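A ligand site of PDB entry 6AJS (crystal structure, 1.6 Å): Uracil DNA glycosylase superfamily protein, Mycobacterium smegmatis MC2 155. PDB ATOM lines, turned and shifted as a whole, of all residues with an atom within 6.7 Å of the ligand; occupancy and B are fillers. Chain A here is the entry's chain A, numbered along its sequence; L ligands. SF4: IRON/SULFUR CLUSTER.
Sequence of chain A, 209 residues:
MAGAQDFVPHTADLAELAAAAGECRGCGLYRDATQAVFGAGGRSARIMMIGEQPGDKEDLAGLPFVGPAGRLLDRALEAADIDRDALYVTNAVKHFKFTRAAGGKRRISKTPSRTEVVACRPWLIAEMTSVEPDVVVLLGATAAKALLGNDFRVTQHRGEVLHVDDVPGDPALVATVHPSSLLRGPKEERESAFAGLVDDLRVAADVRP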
ATOM      1  N   GLY A   3     -10.928  -1.509  15.020  1.00  0.00           N
ATOM      2  CA  GLY A   3     -11.962  -0.605  14.519  1.00  0.00           C
ATOM      3  C   GLY A   3     -12.988  -1.284  13.611  1.00  0.00           C
ATOM      4  O   GLY A   3     -13.549  -2.339  13.943  1.00  0.00           O
ATOM      5  N   ALA A   4     -13.255  -0.653  12.461  1.00  0.00           N
ATOM      6  CA  ALA A   4     -14.234  -1.148  11.505  1.00  0.00           C
ATOM      7  C   ALA A   4     -13.695  -2.211  10.563  1.00  0.00           C
ATOM      8  O   ALA A   4     -14.453  -2.690   9.723  1.00  0.00           O
ATOM      9  CB  ALA A   4     -14.767   0.007  10.643  1.00  0.00           C
ATOM     10  N   PHE A   7     -15.597  -5.331   9.492  1.00  0.00           N
ATOM     11  CA  PHE A   7     -16.904  -5.085   8.925  1.00  0.00           C
ATOM     12  C   PHE A   7     -16.847  -4.700   7.454  1.00  0.00           C
ATOM     13  O   PHE A   7     -17.895  -4.660   6.802  1.00  0.00           O
ATOM     14  CB  PHE A   7     -17.592  -3.966   9.719  1.00  0.00           C
ATOM     15  CG  PHE A   7     -17.926  -4.357  11.128  1.00  0.00           C
ATOM     16  CD1 PHE A   7     -19.050  -5.148  11.396  1.00  0.00           C
ATOM     17  CD2 PHE A   7     -17.130  -3.956  12.174  1.00  0.00           C
ATOM     18  CE1 PHE A   7     -19.363  -5.513  12.703  1.00  0.00           C
ATOM     19  CE2 PHE A   7     -17.441  -4.323  13.491  1.00  0.00           C
ATOM     20  CZ  PHE A   7     -18.551  -5.096  13.739  1.00  0.00           C
ATOM     21  N   ALA A  21     -21.683  -1.126   5.687  1.00  0.00           N
ATOM     22  CA  ALA A  21     -21.505  -0.118   6.720  1.00  0.00           C
ATOM     23  C   ALA A  21     -22.738   0.031   7.600  1.00  0.00           C
ATOM     24  O   ALA A  21     -22.635   0.426   8.766  1.00  0.00           O
ATOM     25  CB  ALA A  21     -21.123   1.226   6.091  1.00  0.00           C
ATOM     26  N   GLU A  23     -24.185  -2.209   8.943  1.00  0.00           N
ATOM     27  CA  GLU A  23     -24.031  -3.194   9.999  1.00  0.00           C
ATOM     28  C   GLU A  23     -22.786  -2.958  10.839  1.00  0.00           C
ATOM     29  O   GLU A  23     -22.477  -3.800  11.695  1.00  0.00           O
ATOM     30  CB  GLU A  23     -23.972  -4.615   9.406  1.00  0.00           C
ATOM     31  CG  GLU A  23     -25.100  -4.949   8.444  1.00  0.00           C
ATOM     32  CD  GLU A  23     -26.460  -4.984   9.108  1.00  0.00           C
ATOM     33  OE1 GLU A  23     -26.504  -5.160  10.346  1.00  0.00           O
ATOM     34  OE2 GLU A  23     -27.477  -4.842   8.396  1.00  0.00           O
ATOM     35  N   CYS A  24     -22.060  -1.867  10.626  1.00  0.00           N
ATOM     36  CA  CYS A  24     -20.799  -1.661  11.323  1.00  0.00           C
ATOM     37  C   CYS A  24     -21.034  -1.361  12.795  1.00  0.00           C
ATOM     38  O   CYS A  24     -21.922  -0.589  13.141  1.00  0.00           O
ATOM     39  CB  CYS A  24     -20.026  -0.511  10.679  1.00  0.00           C
ATOM     40  SG  CYS A  24     -18.352  -0.319  11.357  1.00  0.00           S
ATOM     41  N   ARG A  25     -20.206  -1.964  13.657  1.00  0.00           N
ATOM     42  CA  ARG A  25     -20.159  -1.664  15.076  1.00  0.00           C
ATOM     43  C   ARG A  25     -18.737  -1.341  15.505  1.00  0.00           C
ATOM     44  O   ARG A  25     -18.365  -1.531  16.671  1.00  0.00           O
ATOM     45  CB  ARG A  25     -20.716  -2.816  15.917  1.00  0.00           C
ATOM     46  CG  ARG A  25     -22.124  -3.212  15.545  1.00  0.00           C
ATOM     47  CD  ARG A  25     -22.683  -4.241  16.542  1.00  0.00           C
ATOM     48  NE  ARG A  25     -21.700  -5.281  16.854  1.00  0.00           N
ATOM     49  CZ  ARG A  25     -21.473  -6.319  16.069  1.00  0.00           C
ATOM     50  NH1 ARG A  25     -22.157  -6.432  14.938  1.00  0.00           N
ATOM     51  NH2 ARG A  25     -20.566  -7.231  16.397  1.00  0.00           N
ATOM     52  N   GLY A  26     -17.937  -0.810  14.569  1.00  0.00           N
ATOM     53  CA  GLY A  26     -16.514  -0.612  14.759  1.00  0.00           C
ATOM     54  C   GLY A  26     -16.119   0.375  15.830  1.00  0.00           C
ATOM     55  O   GLY A  26     -14.967   0.377  16.274  1.00  0.00           O
ATOM     56  N   CYS A  27     -17.033   1.229  16.258  1.00  0.00           N
ATOM     57  CA  CYS A  27     -16.847   2.062  17.435  1.00  0.00           C
ATOM     58  C   CYS A  27     -18.202   2.210  18.120  1.00  0.00           C
ATOM     59  O   CYS A  27     -19.175   1.536  17.771  1.00  0.00           O
ATOM     60  CB  CYS A  27     -16.174   3.394  17.069  1.00  0.00           C
ATOM     61  SG  CYS A  27     -17.266   4.616  16.294  1.00  0.00           S
ATOM     62  N   GLY A  28     -18.282   3.087  19.107  1.00  0.00           N
ATOM     63  CA  GLY A  28     -19.569   3.105  19.777  1.00  0.00           C
ATOM     64  C   GLY A  28     -20.633   3.943  19.125  1.00  0.00           C
ATOM     65  O   GLY A  28     -21.783   3.946  19.591  1.00  0.00           O
ATOM     66  N   LEU A  29     -20.300   4.676  18.056  1.00  0.00           N
ATOM     67  CA  LEU A  29     -21.225   5.686  17.542  1.00  0.00           C
ATOM     68  C   LEU A  29     -22.470   5.100  16.889  1.00  0.00           C
ATOM     69  O   LEU A  29     -23.465   5.816  16.719  1.00  0.00           O
ATOM     70  CB  LEU A  29     -20.514   6.580  16.533  1.00  0.00           C
ATOM     71  CG  LEU A  29     -19.390   7.412  17.150  1.00  0.00           C
ATOM     72  CD1 LEU A  29     -18.780   8.324  16.112  1.00  0.00           C
ATOM     73  CD2 LEU A  29     -19.899   8.219  18.340  1.00  0.00           C
ATOM     74  N   TYR A  30     -22.442   3.827  16.502  1.00  0.00           N
ATOM     75  CA  TYR A  30     -23.615   3.251  15.858  1.00  0.00           C
ATOM     76  C   TYR A  30     -24.810   3.184  16.816  1.00  0.00           C
ATOM     77  O   TYR A  30     -25.958   3.103  16.357  1.00  0.00           O
ATOM     78  CB  TYR A  30     -23.313   1.851  15.325  1.00  0.00           C
ATOM     79  CG  TYR A  30     -23.273   0.788  16.410  1.00  0.00           C
ATOM     80  CD1 TYR A  30     -22.126   0.606  17.173  1.00  0.00           C
ATOM     81  CD2 TYR A  30     -24.377   0.001  16.675  1.00  0.00           C
ATOM     82  CE1 TYR A  30     -22.085  -0.326  18.178  1.00  0.00           C
ATOM     83  CE2 TYR A  30     -24.344  -0.951  17.668  1.00  0.00           C
ATOM     84  CZ  TYR A  30     -23.185  -1.105  18.413  1.00  0.00           C
ATOM     85  OH  TYR A  30     -23.150  -2.059  19.415  1.00  0.00           O
ATOM     86  N   ARG A  31     -24.562   3.199  18.135  1.00  0.00           N
ATOM     87  CA  ARG A  31     -25.648   2.888  19.060  1.00  0.00           C
ATOM     88  C   ARG A  31     -26.728   3.970  19.054  1.00  0.00           C
ATOM     89  O   ARG A  31     -27.925   3.656  18.966  1.00  0.00           O
ATOM     90  CB  ARG A  31     -25.091   2.673  20.456  1.00  0.00           C
ATOM     91  CG  ARG A  31     -24.292   1.392  20.574  1.00  0.00           C
ATOM     92  CD  ARG A  31     -24.082   0.998  22.024  1.00  0.00           C
ATOM     93  NE  ARG A  31     -22.705   0.592  22.280  1.00  0.00           N
ATOM     94  CZ  ARG A  31     -21.721   1.450  22.556  1.00  0.00           C
ATOM     95  NH1 ARG A  31     -20.495   1.002  22.782  1.00  0.00           N
ATOM     96  NH2 ARG A  31     -21.975   2.757  22.588  1.00  0.00           N
ATOM     97  N   ALA A  36     -26.051   4.309   9.657  1.00  0.00           N
ATOM     98  CA  ALA A  36     -24.834   4.723   8.994  1.00  0.00           C
ATOM     99  C   ALA A  36     -25.171   5.592   7.786  1.00  0.00           C
ATOM    100  O   ALA A  36     -26.189   5.375   7.104  1.00  0.00           O
ATOM    101  CB  ALA A  36     -24.040   3.498   8.544  1.00  0.00           C
ATOM    102  N   ALA A  92     -15.576  11.542   7.399  1.00  0.00           N
ATOM    103  CA  ALA A  92     -14.519  10.770   8.033  1.00  0.00           C
ATOM    104  C   ALA A  92     -15.090   9.692   8.952  1.00  0.00           C
ATOM    105  O   ALA A  92     -14.521   8.593   9.042  1.00  0.00           O
ATOM    106  CB  ALA A  92     -13.586  11.698   8.816  1.00  0.00           C
ATOM    107  N   VAL A  93     -16.183   9.978   9.653  1.00  0.00           N
ATOM    108  CA  VAL A  93     -16.883   8.930  10.375  1.00  0.00           C
ATOM    109  C   VAL A  93     -18.307   8.885   9.851  1.00  0.00           C
ATOM    110  O   VAL A  93     -18.845   9.881   9.344  1.00  0.00           O
ATOM    111  CB  VAL A  93     -16.869   9.083  11.918  1.00  0.00           C
ATOM    112  CG1 VAL A  93     -15.438   9.251  12.452  1.00  0.00           C
ATOM    113  CG2 VAL A  93     -17.740  10.240  12.371  1.00  0.00           C
ATOM    114  N   LYS A  94     -18.919   7.706   9.943  1.00  0.00           N
ATOM    115  CA  LYS A  94     -20.150   7.438   9.220  1.00  0.00           C
ATOM    116  C   LYS A  94     -21.388   7.378  10.104  1.00  0.00           C
ATOM    117  O   LYS A  94     -22.480   7.177   9.573  1.00  0.00           O
ATOM    118  CB  LYS A  94     -20.012   6.128   8.414  1.00  0.00           C
ATOM    119  CG  LYS A  94     -18.787   6.071   7.480  1.00  0.00           C
ATOM    120  CD  LYS A  94     -19.000   6.783   6.190  1.00  0.00           C
ATOM    121  CE  LYS A  94     -17.989   6.339   5.135  1.00  0.00           C
ATOM    122  NZ  LYS A  94     -16.681   7.142   5.215  1.00  0.00           N
ATOM    123  N   HIS A  95     -21.260   7.560  11.414  1.00  0.00           N
ATOM    124  CA  HIS A  95     -22.403   7.682  12.303  1.00  0.00           C
ATOM    125  C   HIS A  95     -22.370   9.025  13.052  1.00  0.00           C
ATOM    126  O   HIS A  95     -21.316   9.451  13.517  1.00  0.00           O
ATOM    127  CB  HIS A  95     -22.449   6.543  13.329  1.00  0.00           C
ATOM    128  CG  HIS A  95     -22.965   5.244  12.793  1.00  0.00           C
ATOM    129  ND1 HIS A  95     -22.142   4.181  12.490  1.00  0.00           N
ATOM    130  CD2 HIS A  95     -24.223   4.798  12.590  1.00  0.00           C
ATOM    131  CE1 HIS A  95     -22.858   3.165  12.063  1.00  0.00           C
ATOM    132  NE2 HIS A  95     -24.130   3.502  12.126  1.00  0.00           N
ATOM    133  N   PHE A  96     -23.539   9.647  13.177  1.00  0.00           N
ATOM    134  CA  PHE A  96     -23.699  10.946  13.820  1.00  0.00           C
ATOM    135  C   PHE A  96     -23.486  10.821  15.327  1.00  0.00           C
ATOM    136  O   PHE A  96     -24.129  10.002  15.996  1.00  0.00           O
ATOM    137  CB  PHE A  96     -25.102  11.452  13.462  1.00  0.00           C
ATOM    138  CG  PHE A  96     -25.492  12.788  14.072  1.00  0.00           C
ATOM    139  CD1 PHE A  96     -24.629  13.867  14.131  1.00  0.00           C
ATOM    140  CD2 PHE A  96     -26.814  12.952  14.517  1.00  0.00           C
ATOM    141  CE1 PHE A  96     -25.059  15.090  14.657  1.00  0.00           C
ATOM    142  CE2 PHE A  96     -27.254  14.164  15.032  1.00  0.00           C
ATOM    143  CZ  PHE A  96     -26.385  15.230  15.108  1.00  0.00           C
ATOM    144  N   GLU A 116     -12.178   7.340  17.364  1.00  0.00           N
ATOM    145  CA  GLU A 116     -13.292   7.044  16.479  1.00  0.00           C
ATOM    146  C   GLU A 116     -12.931   7.265  15.013  1.00  0.00           C
ATOM    147  O   GLU A 116     -13.266   6.440  14.156  1.00  0.00           O
ATOM    148  CB  GLU A 116     -14.507   7.881  16.878  1.00  0.00           C
ATOM    149  CG  GLU A 116     -15.190   7.323  18.137  1.00  0.00           C
ATOM    150  CD  GLU A 116     -15.941   8.356  18.938  1.00  0.00           C
ATOM    151  OE1 GLU A 116     -15.808   9.578  18.675  1.00  0.00           O
ATOM    152  OE2 GLU A 116     -16.684   7.942  19.862  1.00  0.00           O
ATOM    153  N   ALA A 119     -10.878   4.353  14.005  1.00  0.00           N
ATOM    154  CA  ALA A 119     -11.724   3.162  13.902  1.00  0.00           C
ATOM    155  C   ALA A 119     -12.488   3.145  12.587  1.00  0.00           C
ATOM    156  O   ALA A 119     -12.661   2.078  11.986  1.00  0.00           O
ATOM    157  CB  ALA A 119     -12.711   3.096  15.079  1.00  0.00           C
ATOM    158  N   CYS A 120     -12.979   4.311  12.153  1.00  0.00           N
ATOM    159  CA  CYS A 120     -13.812   4.369  10.968  1.00  0.00           C
ATOM    160  C   CYS A 120     -13.001   4.456   9.683  1.00  0.00           C
ATOM    161  O   CYS A 120     -13.562   4.232   8.593  1.00  0.00           O
ATOM    162  CB  CYS A 120     -14.777   5.564  11.063  1.00  0.00           C
ATOM    163  SG  CYS A 120     -16.298   5.396  10.061  1.00  0.00           S
ATOM    164  N   ARG A 121     -11.719   4.772   9.786  1.00  0.00           N
ATOM    165  CA  ARG A 121     -10.903   4.996   8.597  1.00  0.00           C
ATOM    166  C   ARG A 121     -10.892   3.823   7.622  1.00  0.00           C
ATOM    167  O   ARG A 121     -10.791   4.088   6.411  1.00  0.00           O
ATOM    168  CB  ARG A 121      -9.468   5.381   8.993  1.00  0.00           C
ATOM    169  CG  ARG A 121      -8.746   6.135   7.864  1.00  0.00           C
ATOM    170  CD  ARG A 121      -7.582   6.978   8.413  1.00  0.00           C
ATOM    171  NE  ARG A 121      -6.683   6.135   9.199  1.00  0.00           N
ATOM    172  CZ  ARG A 121      -5.767   6.601  10.038  1.00  0.00           C
ATOM    173  NH1 ARG A 121      -5.621   7.922  10.204  1.00  0.00           N
ATOM    174  NH2 ARG A 121      -4.990   5.769  10.715  1.00  0.00           N
ATOM    175  N   PRO A 122     -11.016   2.554   8.020  1.00  0.00           N
ATOM    176  CA  PRO A 122     -11.112   1.507   6.995  1.00  0.00           C
ATOM    177  C   PRO A 122     -12.202   1.766   5.966  1.00  0.00           C
ATOM    178  O   PRO A 122     -12.005   1.383   4.807  1.00  0.00           O
ATOM    179  CB  PRO A 122     -11.367   0.230   7.808  1.00  0.00           C
ATOM    180  CG  PRO A 122     -10.663   0.494   9.075  1.00  0.00           C
ATOM    181  CD  PRO A 122     -10.851   1.965   9.372  1.00  0.00           C
ATOM    182  N   TRP A 123     -13.314   2.398   6.340  1.00  0.00           N
ATOM    183  CA  TRP A 123     -14.333   2.743   5.354  1.00  0.00           C
ATOM    184  C   TRP A 123     -13.827   3.791   4.370  1.00  0.00           C
ATOM    185  O   TRP A 123     -14.059   3.674   3.154  1.00  0.00           O
ATOM    186  CB  TRP A 123     -15.606   3.237   6.044  1.00  0.00           C
ATOM    187  CG  TRP A 123     -16.318   2.170   6.796  1.00  0.00           C
ATOM    188  CD1 TRP A 123     -16.579   2.168   8.146  1.00  0.00           C
ATOM    189  CD2 TRP A 123     -16.921   0.981   6.254  1.00  0.00           C
ATOM    190  NE1 TRP A 123     -17.267   1.028   8.477  1.00  0.00           N
ATOM    191  CE2 TRP A 123     -17.482   0.272   7.351  1.00  0.00           C
ATOM    192  CE3 TRP A 123     -17.005   0.417   4.972  1.00  0.00           C
ATOM    193  CZ2 TRP A 123     -18.136  -0.936   7.198  1.00  0.00           C
ATOM    194  CZ3 TRP A 123     -17.666  -0.803   4.819  1.00  0.00           C
ATOM    195  CH2 TRP A 123     -18.213  -1.470   5.930  1.00  0.00           C
HETATM  196 FE1  SF4 L   1     -17.640   4.281  11.573  1.00  0.00          FE
HETATM  197 FE2  SF4 L   1     -17.959   3.745  14.173  1.00  0.00          FE
HETATM  198 FE3  SF4 L   1     -18.461   1.854  12.279  1.00  0.00          FE
HETATM  199 FE4  SF4 L   1     -20.055   3.941  12.621  1.00  0.00          FE
HETATM  200  S1  SF4 L   1     -19.699   2.264  14.177  1.00  0.00           S
HETATM  201  S2  SF4 L   1     -19.344   3.149  10.600  1.00  0.00           S
HETATM  202  S3  SF4 L   1     -18.643   5.638  13.078  1.00  0.00           S
HETATM  203  S4  SF4 L   1     -16.451   2.732  12.799  1.00  0.00           S
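The backbone NH of His 95 sits close to a sulfur (S3) of the ligand, at 3.6 Å.
The indole nitrogen (NE1) of Trp 123 lies close to a sulfur (S2) of the ligand, 3.6 Å away.
An iron atom (FE2) of the ligand is bound by the side-chain sulfur (SG) of Cys 27, 2.4 Å away.
The backbone NH of Lys 94 sits close to a sulfur (S3) of the ligand (3.8 Å).
SG of Cys 24 binds FE3 of the ligand (2.4 Å).
An iron atom (FE1) of the ligand is bound by the side-chain sulfur of Cys 120, 2.3 Å away.
N of Cys 27 sits close to S1 of the ligand (3.5 Å).
A sulfur (S1) of the ligand sits close to the backbone NH (N) of Gly 26 (3.6 Å).
An iron atom (FE4) of the ligand is bound by a ring nitrogen (ND1) of His 95.
Residues that only touch the ligand: Ala 4 (3.9 Å), Arg 25 (3.96 Å), Tyr 30 (3.8 Å) and Ala 119 (3.9 Å).
Hydrophobic or aromatic side chains that line the ligand: Ala 4, Tyr 30, His 95 and Trp 123.
Of the 25 residues printed, 11 come within 4 Å of the ligand.
The nearest printed residue that does not touch the ligand is Leu 29 (4.04 Å).
NE2 of His 95 sits at hydrogen-bond distance from N of Ala 36.
The side-chain sulfur of Cys 120 lies close to the backbone NH of Lys 94, 3.5 Å away.
The side-chain sulfur (SG) of Cys 24 lies close to the backbone NH (N) of Gly 26.
The backbone carbonyl oxygen of Ala 119 is in hydrogen-bond range of the backbone NH of Ala 4 (2.8 Å).
The side-chain sulfur (SG) of Cys 27 lies close to the backbone NH (N) of Leu 29 (3.5 Å).
The indole nitrogen (NE1) of Trp 123 lies close to the side-chain sulfur (SG) of Cys 24 (3.4 Å).
The side-chain sulfur (SG) of Cys 120 lies close to the backbone carbonyl oxygen (O) of Ala 92 (3.8 Å).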
